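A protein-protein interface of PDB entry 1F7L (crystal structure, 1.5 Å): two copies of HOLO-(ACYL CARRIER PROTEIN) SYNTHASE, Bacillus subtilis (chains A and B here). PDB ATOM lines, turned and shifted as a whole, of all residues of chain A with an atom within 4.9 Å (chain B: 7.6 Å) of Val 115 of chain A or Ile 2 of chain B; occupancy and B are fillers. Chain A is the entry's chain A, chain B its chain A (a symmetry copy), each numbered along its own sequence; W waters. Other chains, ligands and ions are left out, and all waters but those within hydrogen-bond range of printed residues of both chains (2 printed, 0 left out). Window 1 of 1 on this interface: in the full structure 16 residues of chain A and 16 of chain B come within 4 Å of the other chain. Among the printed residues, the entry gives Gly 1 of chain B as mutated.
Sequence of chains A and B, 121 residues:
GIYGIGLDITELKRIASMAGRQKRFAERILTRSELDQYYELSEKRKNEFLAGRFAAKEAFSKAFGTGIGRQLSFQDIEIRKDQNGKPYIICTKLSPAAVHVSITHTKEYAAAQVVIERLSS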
ATOM      1  N   ILE A   2      32.914 -30.346 -27.735  1.00  0.00           N
ATOM      2  CA  ILE A   2      31.705 -31.110 -27.439  1.00  0.00           C
ATOM      3  C   ILE A   2      31.714 -32.459 -28.149  1.00  0.00           C
ATOM      4  O   ILE A   2      31.907 -32.530 -29.366  1.00  0.00           O
ATOM      5  CB  ILE A   2      30.443 -30.315 -27.852  1.00  0.00           C
ATOM      6  CG1 ILE A   2      30.290 -29.091 -26.942  1.00  0.00           C
ATOM      7  CG2 ILE A   2      29.204 -31.211 -27.785  1.00  0.00           C
ATOM      8  CD1 ILE A   2      29.194 -28.123 -27.380  1.00  0.00           C
ATOM      9  N   GLY A   4      29.041 -34.676 -27.942  1.00  0.00           N
ATOM     10  CA  GLY A   4      27.716 -34.871 -28.509  1.00  0.00           C
ATOM     11  C   GLY A   4      26.614 -34.203 -27.706  1.00  0.00           C
ATOM     12  O   GLY A   4      26.810 -33.852 -26.538  1.00  0.00           O
ATOM     13  N   ILE A   5      25.455 -34.022 -28.345  1.00  0.00           N
ATOM     14  CA  ILE A   5      24.298 -33.423 -27.678  1.00  0.00           C
ATOM     15  C   ILE A   5      23.083 -34.330 -27.886  1.00  0.00           C
ATOM     16  O   ILE A   5      23.045 -35.135 -28.820  1.00  0.00           O
ATOM     17  CB  ILE A   5      23.982 -31.966 -28.199  1.00  0.00           C
ATOM     18  CG1 ILE A   5      23.357 -31.998 -29.599  1.00  0.00           C
ATOM     19  CG2 ILE A   5      25.268 -31.120 -28.181  1.00  0.00           C
ATOM     20  CD1 ILE A   5      22.961 -30.615 -30.129  1.00  0.00           C
ATOM     21  N   VAL A  99      28.334 -35.131 -16.686  1.00  0.00           N
ATOM     22  CA  VAL A  99      27.792 -34.797 -17.996  1.00  0.00           C
ATOM     23  C   VAL A  99      26.647 -33.798 -17.773  1.00  0.00           C
ATOM     24  O   VAL A  99      25.875 -33.944 -16.828  1.00  0.00           O
ATOM     25  CB  VAL A  99      27.286 -36.073 -18.682  1.00  0.00           C
ATOM     26  CG1 VAL A  99      26.445 -35.732 -19.895  1.00  0.00           C
ATOM     27  CG2 VAL A  99      28.478 -36.938 -19.073  1.00  0.00           C
ATOM     28  N   HIS A 100      26.555 -32.783 -18.626  1.00  0.00           N
ATOM     29  CA  HIS A 100      25.527 -31.754 -18.506  1.00  0.00           C
ATOM     30  C   HIS A 100      24.138 -32.250 -18.861  1.00  0.00           C
ATOM     31  O   HIS A 100      23.957 -32.927 -19.866  1.00  0.00           O
ATOM     32  CB  HIS A 100      25.858 -30.577 -19.419  1.00  0.00           C
ATOM     33  CG  HIS A 100      27.105 -29.845 -19.040  1.00  0.00           C
ATOM     34  ND1 HIS A 100      27.152 -28.937 -18.003  1.00  0.00           N
ATOM     35  CD2 HIS A 100      28.355 -29.888 -19.560  1.00  0.00           C
ATOM     36  CE1 HIS A 100      28.377 -28.455 -17.900  1.00  0.00           C
ATOM     37  NE2 HIS A 100      29.126 -29.015 -18.831  1.00  0.00           N
ATOM     38  N   GLN A 113      17.559 -32.380 -21.922  1.00  0.00           N
ATOM     39  CA  GLN A 113      18.635 -32.243 -22.899  1.00  0.00           C
ATOM     40  C   GLN A 113      19.965 -32.569 -22.214  1.00  0.00           C
ATOM     41  O   GLN A 113      20.103 -32.438 -20.994  1.00  0.00           O
ATOM     42  CB  GLN A 113      18.677 -30.839 -23.516  1.00  0.00           C
ATOM     43  CG  GLN A 113      19.072 -29.739 -22.550  1.00  0.00           C
ATOM     44  CD  GLN A 113      19.098 -28.369 -23.198  1.00  0.00           C
ATOM     45  OE1 GLN A 113      19.444 -27.381 -22.553  1.00  0.00           O
ATOM     46  NE2 GLN A 113      18.715 -28.299 -24.473  1.00  0.00           N
ATOM     47  N   VAL A 114      20.935 -33.002 -23.012  1.00  0.00           N
ATOM     48  CA  VAL A 114      22.250 -33.382 -22.514  1.00  0.00           C
ATOM     49  C   VAL A 114      23.366 -32.881 -23.422  1.00  0.00           C
ATOM     50  O   VAL A 114      23.195 -32.780 -24.636  1.00  0.00           O
ATOM     51  CB  VAL A 114      22.374 -34.938 -22.455  1.00  0.00           C
ATOM     52  CG1 VAL A 114      23.832 -35.361 -22.230  1.00  0.00           C
ATOM     53  CG2 VAL A 114      21.472 -35.492 -21.366  1.00  0.00           C
ATOM     54  N   VAL A 115      24.500 -32.542 -22.814  1.00  0.00           N
ATOM     55  CA  VAL A 115      25.685 -32.154 -23.561  1.00  0.00           C
ATOM     56  C   VAL A 115      26.868 -32.873 -22.919  1.00  0.00           C
ATOM     57  O   VAL A 115      27.111 -32.733 -21.718  1.00  0.00           O
ATOM     58  CB  VAL A 115      25.966 -30.640 -23.538  1.00  0.00           C
ATOM     59  CG1 VAL A 115      27.286 -30.361 -24.246  1.00  0.00           C
ATOM     60  CG2 VAL A 115      24.833 -29.870 -24.217  1.00  0.00           C
ATOM     61  N   ILE A 116      27.579 -33.665 -23.719  1.00  0.00           N
ATOM     62  CA  ILE A 116      28.761 -34.398 -23.252  1.00  0.00           C
ATOM     63  C   ILE A 116      29.976 -33.673 -23.823  1.00  0.00           C
ATOM     64  O   ILE A 116      30.068 -33.491 -25.042  1.00  0.00           O
ATOM     65  CB  ILE A 116      28.810 -35.840 -23.805  1.00  0.00           C
ATOM     66  CG1 ILE A 116      27.618 -36.660 -23.300  1.00  0.00           C
ATOM     67  CG2 ILE A 116      30.135 -36.510 -23.391  1.00  0.00           C
ATOM     68  CD1 ILE A 116      27.560 -38.059 -23.908  1.00  0.00           C
ATOM     69  N   GLU A 117      30.909 -33.274 -22.962  1.00  0.00           N
ATOM     70  CA  GLU A 117      32.106 -32.579 -23.441  1.00  0.00           C
ATOM     71  C   GLU A 117      33.219 -33.574 -23.750  1.00  0.00           C
ATOM     72  O   GLU A 117      33.201 -34.702 -23.266  1.00  0.00           O
ATOM     73  CB  GLU A 117      32.595 -31.569 -22.400  1.00  0.00           C
ATOM     74  CG  GLU A 117      31.553 -30.533 -22.016  1.00  0.00           C
ATOM     75  CD  GLU A 117      32.115 -29.407 -21.171  1.00  0.00           C
ATOM     76  OE1 GLU A 117      32.779 -28.510 -21.733  1.00  0.00           O
ATOM     77  OE2 GLU A 117      31.897 -29.420 -19.943  1.00  0.00           O
ATOM     78  N   GLY B   1      35.379 -24.272 -21.708  1.00  0.00           N
ATOM     79  CA  GLY B   1      34.353 -25.355 -21.641  1.00  0.00           C
ATOM     80  C   GLY B   1      32.963 -24.822 -21.341  1.00  0.00           C
ATOM     81  O   GLY B   1      32.677 -23.643 -21.549  1.00  0.00           O
ATOM     82  N   ILE B   2      32.098 -25.694 -20.841  1.00  0.00           N
ATOM     83  CA  ILE B   2      30.727 -25.304 -20.526  1.00  0.00           C
ATOM     84  C   ILE B   2      30.490 -25.279 -19.020  1.00  0.00           C
ATOM     85  O   ILE B   2      30.766 -26.259 -18.322  1.00  0.00           O
ATOM     86  CB  ILE B   2      29.718 -26.270 -21.192  1.00  0.00           C
ATOM     87  CG1 ILE B   2      29.769 -26.090 -22.715  1.00  0.00           C
ATOM     88  CG2 ILE B   2      28.306 -26.020 -20.655  1.00  0.00           C
ATOM     89  CD1 ILE B   2      28.962 -27.127 -23.491  1.00  0.00           C
ATOM     90  N   TYR B   3      29.989 -24.151 -18.523  1.00  0.00           N
ATOM     91  CA  TYR B   3      29.695 -24.011 -17.105  1.00  0.00           C
ATOM     92  C   TYR B   3      28.373 -24.708 -16.774  1.00  0.00           C
ATOM     93  O   TYR B   3      28.256 -25.376 -15.744  1.00  0.00           O
ATOM     94  CB  TYR B   3      29.612 -22.532 -16.715  1.00  0.00           C
ATOM     95  CG  TYR B   3      29.251 -22.317 -15.264  1.00  0.00           C
ATOM     96  CD1 TYR B   3      30.141 -22.665 -14.242  1.00  0.00           C
ATOM     97  CD2 TYR B   3      28.013 -21.785 -14.907  1.00  0.00           C
ATOM     98  CE1 TYR B   3      29.803 -22.488 -12.897  1.00  0.00           C
ATOM     99  CE2 TYR B   3      27.665 -21.603 -13.570  1.00  0.00           C
ATOM    100  CZ  TYR B   3      28.562 -21.957 -12.571  1.00  0.00           C
ATOM    101  OH  TYR B   3      28.207 -21.790 -11.254  1.00  0.00           O
ATOM    102  N   GLY B   4      27.377 -24.554 -17.648  1.00  0.00           N
ATOM    103  CA  GLY B   4      26.095 -25.198 -17.404  1.00  0.00           C
ATOM    104  C   GLY B   4      25.109 -25.026 -18.546  1.00  0.00           C
ATOM    105  O   GLY B   4      25.278 -24.147 -19.398  1.00  0.00           O
ATOM    106  N   ILE B   5      24.080 -25.878 -18.560  1.00  0.00           N
ATOM    107  CA  ILE B   5      23.036 -25.799 -19.584  1.00  0.00           C
ATOM    108  C   ILE B   5      21.669 -25.778 -18.895  1.00  0.00           C
ATOM    109  O   ILE B   5      21.530 -26.211 -17.748  1.00  0.00           O
ATOM    110  CB  ILE B   5      23.105 -26.994 -20.615  1.00  0.00           C
ATOM    111  CG1 ILE B   5      22.611 -28.302 -19.986  1.00  0.00           C
ATOM    112  CG2 ILE B   5      24.543 -27.137 -21.145  1.00  0.00           C
ATOM    113  CD1 ILE B   5      22.586 -29.485 -20.961  1.00  0.00           C
ATOM    114  N   ALA B  63      20.951 -23.315 -15.841  1.00  0.00           N
ATOM    115  CA  ALA B  63      22.335 -23.354 -16.313  1.00  0.00           C
ATOM    116  C   ALA B  63      23.246 -22.730 -15.255  1.00  0.00           C
ATOM    117  O   ALA B  63      24.382 -23.166 -15.076  1.00  0.00           O
ATOM    118  CB  ALA B  63      22.467 -22.598 -17.645  1.00  0.00           C
ATOM    119  N   GLN B 113      16.241 -22.583 -24.391  1.00  0.00           N
ATOM    120  CA  GLN B 113      17.400 -23.289 -23.854  1.00  0.00           C
ATOM    121  C   GLN B 113      18.558 -22.297 -23.711  1.00  0.00           C
ATOM    122  O   GLN B 113      18.617 -21.281 -24.410  1.00  0.00           O
ATOM    123  CB  GLN B 113      17.812 -24.475 -24.734  1.00  0.00           C
ATOM    124  CG  GLN B 113      18.362 -24.086 -26.094  1.00  0.00           C
ATOM    125  CD  GLN B 113      18.754 -25.285 -26.935  1.00  0.00           C
ATOM    126  OE1 GLN B 113      19.258 -25.130 -28.046  1.00  0.00           O
ATOM    127  NE2 GLN B 113      18.506 -26.490 -26.417  1.00  0.00           N
ATOM    128  N   VAL B 114      19.470 -22.601 -22.793  1.00  0.00           N
ATOM    129  CA  VAL B 114      20.616 -21.747 -22.514  1.00  0.00           C
ATOM    130  C   VAL B 114      21.890 -22.559 -22.314  1.00  0.00           C
ATOM    131  O   VAL B 114      21.852 -23.685 -21.821  1.00  0.00           O
ATOM    132  CB  VAL B 114      20.379 -20.941 -21.197  1.00  0.00           C
ATOM    133  CG1 VAL B 114      21.678 -20.275 -20.723  1.00  0.00           C
ATOM    134  CG2 VAL B 114      19.284 -19.909 -21.409  1.00  0.00           C
ATOM    135  N   VAL B 115      23.015 -21.983 -22.732  1.00  0.00           N
ATOM    136  CA  VAL B 115      24.317 -22.589 -22.505  1.00  0.00           C
ATOM    137  C   VAL B 115      25.246 -21.476 -22.029  1.00  0.00           C
ATOM    138  O   VAL B 115      25.411 -20.461 -22.711  1.00  0.00           O
ATOM    139  CB  VAL B 115      24.930 -23.229 -23.764  1.00  0.00           C
ATOM    140  CG1 VAL B 115      26.335 -23.727 -23.444  1.00  0.00           C
ATOM    141  CG2 VAL B 115      24.064 -24.389 -24.257  1.00  0.00           C
ATOM    142  N   ILE B 116      25.825 -21.661 -20.844  1.00  0.00           N
ATOM    143  CA  ILE B 116      26.766 -20.693 -20.270  1.00  0.00           C
ATOM    144  C   ILE B 116      28.158 -21.301 -20.413  1.00  0.00           C
ATOM    145  O   ILE B 116      28.393 -22.421 -19.946  1.00  0.00           O
ATOM    146  CB  ILE B 116      26.534 -20.482 -18.757  1.00  0.00           C
ATOM    147  CG1 ILE B 116      25.149 -19.882 -18.495  1.00  0.00           C
ATOM    148  CG2 ILE B 116      27.632 -19.562 -18.187  1.00  0.00           C
ATOM    149  CD1 ILE B 116      24.827 -19.758 -17.007  1.00  0.00           C
ATOM    150  N   GLU B 117      29.080 -20.572 -21.039  1.00  0.00           N
ATOM    151  CA  GLU B 117      30.440 -21.090 -21.206  1.00  0.00           C
ATOM    152  C   GLU B 117      31.320 -20.680 -20.031  1.00  0.00           C
ATOM    153  O   GLU B 117      31.006 -19.736 -19.315  1.00  0.00           O
ATOM    154  CB  GLU B 117      31.054 -20.577 -22.511  1.00  0.00           C
ATOM    155  CG  GLU B 117      30.245 -20.928 -23.748  1.00  0.00           C
ATOM    156  CD  GLU B 117      30.973 -20.625 -25.043  1.00  0.00           C
ATOM    157  OE1 GLU B 117      31.869 -21.408 -25.424  1.00  0.00           O
ATOM    158  OE2 GLU B 117      30.654 -19.601 -25.678  1.00  0.00           O
ATOM    159  N   ARG B 118      32.421 -21.396 -19.827  1.00  0.00           N
ATOM    160  CA  ARG B 118      33.323 -21.071 -18.727  1.00  0.00           C
ATOM    161  C   ARG B 118      33.871 -19.658 -18.889  1.00  0.00           C
ATOM    162  O   ARG B 118      33.969 -19.197 -20.048  1.00  0.00           O
ATOM    163  CB  ARG B 118      34.467 -22.072 -18.683  1.00  0.00           C
HETATM  164  O   HOH W   1      24.633 -28.159 -16.692  1.00  0.00           O
HETATM  165  O   HOH W   2      21.024 -25.645 -23.523  1.00  0.00           O
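NE2 of His 100 of chain A sits at hydrogen-bond distance from O of Ile 2 of chain B, 3.2 Å away. The side-chain amide nitrogen (NE2) of Gln 113 of chain A sits close to the side-chain amide nitrogen (NE2) of Gln 113 of chain B (2.7 Å). The side-chain carboxylate (OE1) of Glu 117 of chain A is in hydrogen-bond range of the backbone NH (N) of Ile 2 of chain B (3.0 Å).
The backbone carbonyl oxygen (O) of His 100 of chain A is in hydrogen-bond range of the backbone NH (N) of Val 115 of chain A (3.0 Å). NE2 of His 100 of chain A sits at hydrogen-bond distance from OE2 of Glu 117 of chain A. O of Gly 1 of chain B sits at hydrogen-bond distance from N of Arg 118 of chain B. The backbone carbonyl oxygen (O) of Ile 116 of chain B sits at hydrogen-bond distance from the backbone NH (N) of Tyr 3 of chain B, at 2.8 Å. N of Ile 116 of chain B lies within hydrogen-bond range of O of Gly 4 of chain B (2.9 Å).
Tyr 3 of chain B touches His 100 of chain A (O to CE1, 3.8 Å). ND1 of His 100 of chain A touches CA of Gly 4 of chain B (3.9 Å). CD1 of Ile 5 of chain B touches CB of His 100 of chain A, at 3.8 Å. Gln 113 of chain A touches Ile 5 of chain B (O to CD1, 3.9 Å). CD1 of Ile 2 of chain B touches CG1 of Val 115 of chain A, at 3.7 Å. Val 115 of chain A touches Ile 5 of chain B (CG2 to CD1, 3.97 Å). OE1 of Glu 117 of chain A touches CA of Gly 1 of chain B, at 3.5 Å.
Gly 4 of chain A touches none of the printed residues of chain B. Val 99 of chain A touches none of the printed residues of chain B. Of the printed residues of chain B, Gln 113 of chain A touches Ile 5 and Gln 113. Val 115 of chain A touches two residues of chain B. Ile 2 of chain B touches three residues of chain A. Printed residues of chain A within 4 Å of Tyr 3 of chain B: His 100. Printed residues of chain A within 4 Å of Gly 4 of chain B: His 100. Printed residues of chain A within 4 Å of Ile 5 of chain B: His 100, Gln 113 and Val 115. Printed residues of chain A within 4 Å of Gln 113 of chain B: Gln 113. The nearest residue of chain B that does not touch Val 115 of chain A is Val 115 of chain B (5.5 Å). The nearest residue of chain A that does not touch Ile 2 of chain B is Ile 2 of chain A (4.02 Å).
Hydrophobic or aromatic side chains of chain B within 4 Å of the printed part of chain A: Ile 2 and Ile 5. Of the 10 printed residues of chain A, 4 touch a printed residue of chain B. Printed residues of chain A that touch a printed residue of chain B: His 100, Gln 113, Val 115 and Glu 117. Among the printed residues, 10 pairs touch across the chains. Among the printed residues, no Asp or Glu carboxylate lies within 4 Å of a Lys or Arg side-chain nitrogen of the other chain.
Gln 113 of chain A touches Ile 5 of chain B, but with the chains exchanged Ile 5 of chain A does not touch Gln 113 of chain B (6.9 Å). Gln 113 of chain B touches its own counterpart, Gln 113 of chain A. Val 115 of chain A touches Ile 2 of chain B, but with the chains exchanged Ile 2 of chain A does not touch Val 115 of chain B (6.6 Å). Val 115 of chain A touches Ile 5 of chain B, but with the chains exchanged Ile 5 of chain A does not touch Val 115 of chain B (7.9 Å). Positions printed for both chains: 2, 4, 5, 113, 114, 115, 116 and 117. Of the 10 pairs that touch across the chains among the printed residues, 1 has its exchanged pair printed and touching as well.
Water W2 lies within hydrogen-bond range of OE1 of Gln 113 of chain A (2.5 Å) and O of Val 114 of chain B (2.7 Å). Water W1 lies within hydrogen-bond range of ND1 of His 100 of chain A (2.9 Å) and N of Ile 5 of chain B (3.0 Å).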
